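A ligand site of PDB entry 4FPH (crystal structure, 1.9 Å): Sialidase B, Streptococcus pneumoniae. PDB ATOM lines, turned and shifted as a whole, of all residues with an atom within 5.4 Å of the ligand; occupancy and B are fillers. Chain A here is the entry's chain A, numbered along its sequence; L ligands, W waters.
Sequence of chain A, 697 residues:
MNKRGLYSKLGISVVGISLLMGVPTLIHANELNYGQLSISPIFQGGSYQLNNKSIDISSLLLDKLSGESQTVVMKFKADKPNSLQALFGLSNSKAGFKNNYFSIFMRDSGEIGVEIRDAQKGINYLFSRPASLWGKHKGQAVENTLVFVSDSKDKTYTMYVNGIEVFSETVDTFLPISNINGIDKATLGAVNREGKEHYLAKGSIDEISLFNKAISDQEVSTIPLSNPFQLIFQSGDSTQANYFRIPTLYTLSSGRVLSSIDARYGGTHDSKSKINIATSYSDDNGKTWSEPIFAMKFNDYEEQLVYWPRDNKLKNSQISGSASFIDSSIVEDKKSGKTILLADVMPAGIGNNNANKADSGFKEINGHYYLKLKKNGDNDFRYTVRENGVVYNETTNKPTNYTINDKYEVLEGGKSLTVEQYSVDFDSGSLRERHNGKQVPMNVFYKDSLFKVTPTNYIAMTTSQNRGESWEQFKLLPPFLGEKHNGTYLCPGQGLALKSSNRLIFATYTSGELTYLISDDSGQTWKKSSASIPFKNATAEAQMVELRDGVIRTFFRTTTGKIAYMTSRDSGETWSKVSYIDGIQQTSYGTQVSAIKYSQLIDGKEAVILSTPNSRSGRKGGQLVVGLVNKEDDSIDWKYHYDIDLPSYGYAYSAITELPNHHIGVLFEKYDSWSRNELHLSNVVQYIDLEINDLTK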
ATOM      1  N   ARG A 245     -16.969  -3.829   3.057  1.00  0.00           N
ATOM      2  CA  ARG A 245     -15.953  -3.574   4.073  1.00  0.00           C
ATOM      3  C   ARG A 245     -16.436  -4.119   5.393  1.00  0.00           C
ATOM      4  O   ARG A 245     -17.634  -4.385   5.544  1.00  0.00           O
ATOM      5  CB  ARG A 245     -15.656  -2.071   4.188  1.00  0.00           C
ATOM      6  CG  ARG A 245     -14.563  -1.533   3.233  1.00  0.00           C
ATOM      7  CD  ARG A 245     -13.794  -0.341   3.845  1.00  0.00           C
ATOM      8  NE  ARG A 245     -13.044  -0.740   5.040  1.00  0.00           N
ATOM      9  CZ  ARG A 245     -12.468   0.114   5.874  1.00  0.00           C
ATOM     10  NH1 ARG A 245     -12.527   1.426   5.658  1.00  0.00           N
ATOM     11  NH2 ARG A 245     -11.817  -0.352   6.937  1.00  0.00           N
ATOM     12  N   ILE A 246     -15.526  -4.265   6.352  1.00  0.00           N
ATOM     13  CA  ILE A 246     -15.882  -4.578   7.748  1.00  0.00           C
ATOM     14  C   ILE A 246     -16.504  -5.975   7.907  1.00  0.00           C
ATOM     15  O   ILE A 246     -17.648  -6.105   8.351  1.00  0.00           O
ATOM     16  CB  ILE A 246     -16.814  -3.485   8.401  1.00  0.00           C
ATOM     17  CG1 ILE A 246     -16.511  -2.070   7.892  1.00  0.00           C
ATOM     18  CG2 ILE A 246     -16.708  -3.508   9.916  1.00  0.00           C
ATOM     19  CD1 ILE A 246     -15.112  -1.518   8.231  1.00  0.00           C
ATOM     20  N   ASP A 270     -16.659   5.318   4.262  1.00  0.00           N
ATOM     21  CA  ASP A 270     -17.495   5.214   5.475  1.00  0.00           C
ATOM     22  C   ASP A 270     -18.715   6.129   5.286  1.00  0.00           C
ATOM     23  O   ASP A 270     -18.717   6.991   4.406  1.00  0.00           O
ATOM     24  CB  ASP A 270     -16.788   5.725   6.741  1.00  0.00           C
ATOM     25  CG  ASP A 270     -15.680   4.811   7.233  1.00  0.00           C
ATOM     26  OD1 ASP A 270     -14.904   5.281   8.095  1.00  0.00           O
ATOM     27  OD2 ASP A 270     -15.581   3.653   6.780  1.00  0.00           O
ATOM     28  N   SER A 271     -19.719   5.958   6.139  1.00  0.00           N
ATOM     29  CA  SER A 271     -20.805   6.942   6.247  1.00  0.00           C
ATOM     30  C   SER A 271     -20.213   8.363   6.386  1.00  0.00           C
ATOM     31  O   SER A 271     -19.158   8.514   6.972  1.00  0.00           O
ATOM     32  CB  SER A 271     -21.645   6.624   7.472  1.00  0.00           C
ATOM     33  OG  SER A 271     -22.150   5.296   7.391  1.00  0.00           O
ATOM     34  N   LYS A 272     -20.868   9.402   5.857  1.00  0.00           N
ATOM     35  CA  LYS A 272     -22.136   9.325   5.114  1.00  0.00           C
ATOM     36  C   LYS A 272     -22.030   8.601   3.767  1.00  0.00           C
ATOM     37  O   LYS A 272     -21.111   8.822   2.982  1.00  0.00           O
ATOM     38  CB  LYS A 272     -22.693  10.752   4.884  1.00  0.00           C
ATOM     39  CG  LYS A 272     -21.789  11.641   4.027  1.00  0.00           C
ATOM     40  CD  LYS A 272     -22.351  13.051   3.849  1.00  0.00           C
ATOM     41  CE  LYS A 272     -21.385  13.944   3.046  1.00  0.00           C
ATOM     42  NZ  LYS A 272     -21.834  15.379   2.987  1.00  0.00           N
ATOM     43  N   ILE A 326     -23.495   0.824   9.676  1.00  0.00           N
ATOM     44  CA  ILE A 326     -22.051   0.635   9.534  1.00  0.00           C
ATOM     45  C   ILE A 326     -21.503  -0.061  10.764  1.00  0.00           C
ATOM     46  O   ILE A 326     -21.990   0.172  11.859  1.00  0.00           O
ATOM     47  CB  ILE A 326     -21.337   1.996   9.235  1.00  0.00           C
ATOM     48  CG1 ILE A 326     -19.819   1.839   9.166  1.00  0.00           C
ATOM     49  CG2 ILE A 326     -21.716   3.079  10.238  1.00  0.00           C
ATOM     50  CD1 ILE A 326     -19.144   3.088   8.553  1.00  0.00           C
ATOM     51  N   ASP A 327     -20.514  -0.929  10.575  1.00  0.00           N
ATOM     52  CA  ASP A 327     -19.842  -1.645  11.667  1.00  0.00           C
ATOM     53  C   ASP A 327     -20.771  -2.608  12.419  1.00  0.00           C
ATOM     54  O   ASP A 327     -21.317  -2.264  13.468  1.00  0.00           O
ATOM     55  CB  ASP A 327     -19.205  -0.677  12.675  1.00  0.00           C
ATOM     56  CG  ASP A 327     -17.992   0.061  12.122  1.00  0.00           C
ATOM     57  OD1 ASP A 327     -17.521  -0.268  11.015  1.00  0.00           O
ATOM     58  OD2 ASP A 327     -17.496   0.985  12.821  1.00  0.00           O
ATOM     59  N   ASP A 344     -23.890   0.186  14.000  1.00  0.00           N
ATOM     60  CA  ASP A 344     -24.156   1.613  14.149  1.00  0.00           C
ATOM     61  C   ASP A 344     -25.251   2.020  13.156  1.00  0.00           C
ATOM     62  O   ASP A 344     -25.385   1.410  12.080  1.00  0.00           O
ATOM     63  CB  ASP A 344     -22.921   2.479  13.855  1.00  0.00           C
ATOM     64  CG  ASP A 344     -21.734   2.176  14.763  1.00  0.00           C
ATOM     65  OD1 ASP A 344     -21.911   1.726  15.907  1.00  0.00           O
ATOM     66  OD2 ASP A 344     -20.591   2.432  14.316  1.00  0.00           O
ATOM     67  N   MET A 346     -26.782   5.487  11.114  1.00  0.00           N
ATOM     68  CA  MET A 346     -26.525   6.880  10.764  1.00  0.00           C
ATOM     69  C   MET A 346     -27.720   7.436   9.999  1.00  0.00           C
ATOM     70  O   MET A 346     -28.142   6.864   8.996  1.00  0.00           O
ATOM     71  CB  MET A 346     -25.277   6.982   9.877  1.00  0.00           C
ATOM     72  CG  MET A 346     -24.065   6.254  10.429  1.00  0.00           C
ATOM     73  SD  MET A 346     -23.218   7.246  11.665  1.00  0.00           S
ATOM     74  CE  MET A 346     -22.691   5.923  12.749  1.00  0.00           C
ATOM     75  N   GLY A 351     -22.253  10.943   9.169  1.00  0.00           N
ATOM     76  CA  GLY A 351     -21.136  10.042   9.399  1.00  0.00           C
ATOM     77  C   GLY A 351     -20.494  10.387  10.737  1.00  0.00           C
ATOM     78  O   GLY A 351     -21.055  11.179  11.504  1.00  0.00           O
ATOM     79  N   ASN A 352     -19.323   9.816  11.047  1.00  0.00           N
ATOM     80  CA  ASN A 352     -18.701  10.135  12.336  1.00  0.00           C
ATOM     81  C   ASN A 352     -18.117  11.553  12.363  1.00  0.00           C
ATOM     82  O   ASN A 352     -17.978  12.148  13.431  1.00  0.00           O
ATOM     83  CB  ASN A 352     -17.706   9.053  12.817  1.00  0.00           C
ATOM     84  CG  ASN A 352     -16.338   9.113  12.137  1.00  0.00           C
ATOM     85  OD1 ASN A 352     -16.078   9.959  11.281  1.00  0.00           O
ATOM     86  ND2 ASN A 352     -15.446   8.198  12.531  1.00  0.00           N
ATOM     87  N   ASN A 353     -17.817  12.069  11.173  1.00  0.00           N
ATOM     88  CA  ASN A 353     -17.281  13.433  11.010  1.00  0.00           C
ATOM     89  C   ASN A 353     -18.263  14.539  11.416  1.00  0.00           C
ATOM     90  O   ASN A 353     -17.883  15.514  12.079  1.00  0.00           O
ATOM     91  CB  ASN A 353     -16.803  13.641   9.564  1.00  0.00           C
ATOM     92  CG  ASN A 353     -16.841  15.100   9.122  1.00  0.00           C
ATOM     93  OD1 ASN A 353     -16.055  15.930   9.593  1.00  0.00           O
ATOM     94  ND2 ASN A 353     -17.738  15.424   8.186  1.00  0.00           N
ATOM     95  N   TYR A 489     -19.488   3.993  19.670  1.00  0.00           N
ATOM     96  CA  TYR A 489     -19.350   3.323  18.381  1.00  0.00           C
ATOM     97  C   TYR A 489     -19.103   1.849  18.589  1.00  0.00           C
ATOM     98  O   TYR A 489     -18.176   1.461  19.303  1.00  0.00           O
ATOM     99  CB  TYR A 489     -18.204   3.956  17.580  1.00  0.00           C
ATOM    100  CG  TYR A 489     -18.527   5.340  17.082  1.00  0.00           C
ATOM    101  CD1 TYR A 489     -19.166   5.515  15.860  1.00  0.00           C
ATOM    102  CD2 TYR A 489     -18.226   6.467  17.824  1.00  0.00           C
ATOM    103  CE1 TYR A 489     -19.487   6.763  15.387  1.00  0.00           C
ATOM    104  CE2 TYR A 489     -18.538   7.732  17.360  1.00  0.00           C
ATOM    105  CZ  TYR A 489     -19.174   7.872  16.142  1.00  0.00           C
ATOM    106  OH  TYR A 489     -19.498   9.107  15.639  1.00  0.00           O
ATOM    107  N   TYR A 509     -16.667   1.784  21.563  1.00  0.00           N
ATOM    108  CA  TYR A 509     -15.675   2.781  21.953  1.00  0.00           C
ATOM    109  C   TYR A 509     -16.213   4.208  21.916  1.00  0.00           C
ATOM    110  O   TYR A 509     -17.148   4.532  21.178  1.00  0.00           O
ATOM    111  CB  TYR A 509     -14.381   2.667  21.124  1.00  0.00           C
ATOM    112  CG  TYR A 509     -14.549   2.943  19.637  1.00  0.00           C
ATOM    113  CD1 TYR A 509     -14.348   4.207  19.105  1.00  0.00           C
ATOM    114  CD2 TYR A 509     -14.880   1.917  18.761  1.00  0.00           C
ATOM    115  CE1 TYR A 509     -14.501   4.460  17.753  1.00  0.00           C
ATOM    116  CE2 TYR A 509     -15.024   2.142  17.403  1.00  0.00           C
ATOM    117  CZ  TYR A 509     -14.821   3.418  16.899  1.00  0.00           C
ATOM    118  OH  TYR A 509     -14.975   3.649  15.550  1.00  0.00           O
ATOM    119  N   THR A 539      -9.975   5.619  17.550  1.00  0.00           N
ATOM    120  CA  THR A 539     -10.846   4.590  16.983  1.00  0.00           C
ATOM    121  C   THR A 539     -10.428   3.303  17.680  1.00  0.00           C
ATOM    122  O   THR A 539      -9.672   2.509  17.142  1.00  0.00           O
ATOM    123  CB  THR A 539     -10.641   4.486  15.457  1.00  0.00           C
ATOM    124  OG1 THR A 539     -10.842   5.773  14.858  1.00  0.00           O
ATOM    125  CG2 THR A 539     -11.618   3.501  14.845  1.00  0.00           C
ATOM    126  N   GLU A 541     -11.180   0.234  18.330  1.00  0.00           N
ATOM    127  CA  GLU A 541     -11.914  -0.972  17.984  1.00  0.00           C
ATOM    128  C   GLU A 541     -11.345  -2.141  18.793  1.00  0.00           C
ATOM    129  O   GLU A 541     -10.151  -2.403  18.748  1.00  0.00           O
ATOM    130  CB  GLU A 541     -11.832  -1.235  16.475  1.00  0.00           C
ATOM    131  CG  GLU A 541     -12.563  -0.139  15.641  1.00  0.00           C
ATOM    132  CD  GLU A 541     -12.041  -0.034  14.220  1.00  0.00           C
ATOM    133  OE1 GLU A 541     -12.784   0.460  13.339  1.00  0.00           O
ATOM    134  OE2 GLU A 541     -10.882  -0.448  13.998  1.00  0.00           O
ATOM    135  N   ARG A 557      -7.327  -1.543  19.042  1.00  0.00           N
ATOM    136  CA  ARG A 557      -6.626  -0.611  18.163  1.00  0.00           C
ATOM    137  C   ARG A 557      -6.313   0.670  18.929  1.00  0.00           C
ATOM    138  O   ARG A 557      -7.136   1.149  19.698  1.00  0.00           O
ATOM    139  CB  ARG A 557      -7.537  -0.295  16.973  1.00  0.00           C
ATOM    140  CG  ARG A 557      -7.002   0.720  15.960  1.00  0.00           C
ATOM    141  CD  ARG A 557      -8.080   0.978  14.925  1.00  0.00           C
ATOM    142  NE  ARG A 557      -7.807   2.149  14.085  1.00  0.00           N
ATOM    143  CZ  ARG A 557      -8.478   2.417  12.972  1.00  0.00           C
ATOM    144  NH1 ARG A 557      -9.446   1.588  12.566  1.00  0.00           N
ATOM    145  NH2 ARG A 557      -8.171   3.498  12.276  1.00  0.00           N
ATOM    146  N   GLY A 590      -3.721   2.972  13.024  1.00  0.00           N
ATOM    147  CA  GLY A 590      -4.162   1.678  13.520  1.00  0.00           C
ATOM    148  C   GLY A 590      -5.150   0.956  12.617  1.00  0.00           C
ATOM    149  O   GLY A 590      -5.658   1.521  11.647  1.00  0.00           O
ATOM    150  N   ARG A 619      -1.585  -0.647   5.728  1.00  0.00           N
ATOM    151  CA  ARG A 619      -2.381  -1.834   6.062  1.00  0.00           C
ATOM    152  C   ARG A 619      -1.986  -2.958   5.105  1.00  0.00           C
ATOM    153  O   ARG A 619      -2.554  -3.122   4.026  1.00  0.00           O
ATOM    154  CB  ARG A 619      -3.885  -1.509   6.023  1.00  0.00           C
ATOM    155  CG  ARG A 619      -4.305  -0.469   7.068  1.00  0.00           C
ATOM    156  CD  ARG A 619      -5.788  -0.197   7.087  1.00  0.00           C
ATOM    157  NE  ARG A 619      -6.212   0.445   8.335  1.00  0.00           N
ATOM    158  CZ  ARG A 619      -7.370   1.062   8.516  1.00  0.00           C
ATOM    159  NH1 ARG A 619      -8.246   1.130   7.508  1.00  0.00           N
ATOM    160  NH2 ARG A 619      -7.667   1.618   9.673  1.00  0.00           N
ATOM    161  N   TYR A 653      -9.018  -4.723   7.728  1.00  0.00           N
ATOM    162  CA  TYR A 653      -9.953  -5.255   8.727  1.00  0.00           C
ATOM    163  C   TYR A 653     -10.108  -6.741   8.479  1.00  0.00           C
ATOM    164  O   TYR A 653     -10.002  -7.201   7.337  1.00  0.00           O
ATOM    165  CB  TYR A 653     -11.316  -4.575   8.652  1.00  0.00           C
ATOM    166  CG  TYR A 653     -11.391  -3.243   9.350  1.00  0.00           C
ATOM    167  CD1 TYR A 653     -10.386  -2.297   9.211  1.00  0.00           C
ATOM    168  CD2 TYR A 653     -12.489  -2.909  10.132  1.00  0.00           C
ATOM    169  CE1 TYR A 653     -10.456  -1.064   9.830  1.00  0.00           C
ATOM    170  CE2 TYR A 653     -12.577  -1.667  10.748  1.00  0.00           C
ATOM    171  CZ  TYR A 653     -11.563  -0.749  10.593  1.00  0.00           C
ATOM    172  OH  TYR A 653     -11.661   0.475  11.210  1.00  0.00           O
ATOM    173  N   SER A 673      -7.254  -0.513   3.094  1.00  0.00           N
ATOM    174  CA  SER A 673      -8.498   0.260   3.180  1.00  0.00           C
ATOM    175  C   SER A 673      -8.302   1.634   3.837  1.00  0.00           C
ATOM    176  O   SER A 673      -9.283   2.332   4.134  1.00  0.00           O
ATOM    177  CB  SER A 673      -9.593  -0.532   3.901  1.00  0.00           C
ATOM    178  OG  SER A 673      -9.196  -0.854   5.210  1.00  0.00           O
ATOM    179  N   TRP A 674      -7.050   2.031   4.059  1.00  0.00           N
ATOM    180  CA  TRP A 674      -6.768   3.401   4.491  1.00  0.00           C
ATOM    181  C   TRP A 674      -6.317   4.210   3.281  1.00  0.00           C
ATOM    182  O   TRP A 674      -6.739   5.370   3.102  1.00  0.00           O
ATOM    183  CB  TRP A 674      -5.675   3.412   5.569  1.00  0.00           C
ATOM    184  CG  TRP A 674      -5.426   4.788   6.179  1.00  0.00           C
ATOM    185  CD1 TRP A 674      -4.463   5.696   5.789  1.00  0.00           C
ATOM    186  CD2 TRP A 674      -6.133   5.394   7.267  1.00  0.00           C
ATOM    187  NE1 TRP A 674      -4.543   6.830   6.579  1.00  0.00           N
ATOM    188  CE2 TRP A 674      -5.553   6.666   7.491  1.00  0.00           C
ATOM    189  CE3 TRP A 674      -7.191   4.988   8.080  1.00  0.00           C
ATOM    190  CZ2 TRP A 674      -6.006   7.528   8.502  1.00  0.00           C
ATOM    191  CZ3 TRP A 674      -7.641   5.835   9.082  1.00  0.00           C
ATOM    192  CH2 TRP A 674      -7.054   7.091   9.279  1.00  0.00           C
HETATM  193  O1  LIG L   1     -10.137   3.120  10.044  1.00  0.00           O
HETATM  194  S1  LIG L   1     -11.085   3.230   8.894  1.00  0.00           S
HETATM  195  O2  LIG L   1     -10.715   2.318   7.801  1.00  0.00           O
HETATM  196  O3  LIG L   1     -11.087   4.607   8.363  1.00  0.00           O
HETATM  197  C1  LIG L   1     -12.765   2.853   9.431  1.00  0.00           C
HETATM  198  C2  LIG L   1     -13.335   3.629  10.602  1.00  0.00           C
HETATM  199  N1  LIG L   1     -14.758   3.871  10.488  1.00  0.00           N
HETATM  200  C3  LIG L   1     -15.290   4.490  11.680  1.00  0.00           C
HETATM  201  C4  LIG L   1     -16.735   4.873  11.610  1.00  0.00           C
HETATM  202  C5  LIG L   1     -17.139   5.866  10.743  1.00  0.00           C
HETATM  203  C6  LIG L   1     -18.500   6.214  10.674  1.00  0.00           C
HETATM  204  F1  LIG L   1     -18.930   7.168   9.839  1.00  0.00           F
HETATM  205  C7  LIG L   1     -19.426   5.530  11.508  1.00  0.00           C
HETATM  206  C8  LIG L   1     -19.014   4.532  12.385  1.00  0.00           C
HETATM  207  C9  LIG L   1     -17.683   4.189  12.442  1.00  0.00           C
HETATM  208  O   HOH W   1     -15.008   1.810  13.817  1.00  0.00           O
HETATM  209  O   HOH W   2     -15.629   1.430   9.850  1.00  0.00           O
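The guanidinium group of Arg 619 lies within salt-bridge range of an oxygen (O2) of the ligand, 2.8 Å away. A nitrogen (N1) of the ligand is in salt-bridge range of the side-chain carboxylate of Asp 270 (2.8 Å). The guanidinium group (NH1) of Arg 245 lies within salt-bridge range of an oxygen (O2) of the ligand (2.9 Å). NH2 of Arg 557 lies within salt-bridge range of O1 of the ligand, at 3.0 Å. The side-chain hydroxyl of Tyr 653 lies close to an oxygen (O1) of the ligand (3.3 Å).
The guanidinium group (NH1) of Arg 619 is in hydrogen-bond range of the side-chain hydroxyl (OG) of Ser 673, at 3.2 Å. O of Gly 590 lies within hydrogen-bond range of NH2 of Arg 619, 2.8 Å away. The side-chain carboxylate (OD2) of Asp 270 is in salt-bridge range of the guanidinium group (NH1) of Arg 245 (3.9 Å). NH1 of Arg 557 is in hydrogen-bond range of OH of Tyr 653 (2.8 Å). The backbone carbonyl oxygen of Gly 590 sits close to the guanidinium group of Arg 557, 3.3 Å away. The side-chain hydroxyl (OH) of Tyr 653 is in hydrogen-bond range of the side-chain carboxylate (OE1) of Glu 541 (2.4 Å). The backbone carbonyl oxygen (O) of Ile 326 sits at hydrogen-bond distance from the backbone NH (N) of Asp 344 (2.9 Å). O of Tyr 489 is in hydrogen-bond range of N of Tyr 509 (2.7 Å).
F1 of the ligand lies close to O of Ser 271 (3.2 Å). The backbone NH of Asn 352 lies close to a fluorine (F1) of the ligand (2.9 Å). CG2 of Ile 326 touches C7 of the ligand (3.6 Å). OD2 of Asp 327 touches C9 of the ligand (3.2 Å). OD2 of Asp 344 touches C8 of the ligand, at 3.3 Å. Met 346 touches the ligand (CE to C7, 3.5 Å). Gly 351 touches the ligand (CA to F1, 3.6 Å). Tyr 489 touches the ligand. OH of Tyr 509 touches C3 of the ligand (3.97 Å). Ser 673 touches the ligand. Trp 674 touches the ligand (CZ3 to O3, 3.7 Å). Hydrophobic or aromatic side chains that line the ligand: Ile 326, Met 346, Tyr 489, Tyr 653 and Trp 674. Of the 22 residues printed, 16 come within 4 Å of the ligand. The nearest printed residue that does not touch the ligand is Glu 541 (4.2 Å).
Water W2 lies within hydrogen-bond range of N1 of the ligand (2.7 Å) and OD1 of Asp 327 (2.8 Å). Water W1 lies within hydrogen-bond range of OH of Tyr 509 (2.5 Å), OE1 of Glu 541 (2.6 Å) and OD2 of Asp 327 (2.8 Å).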
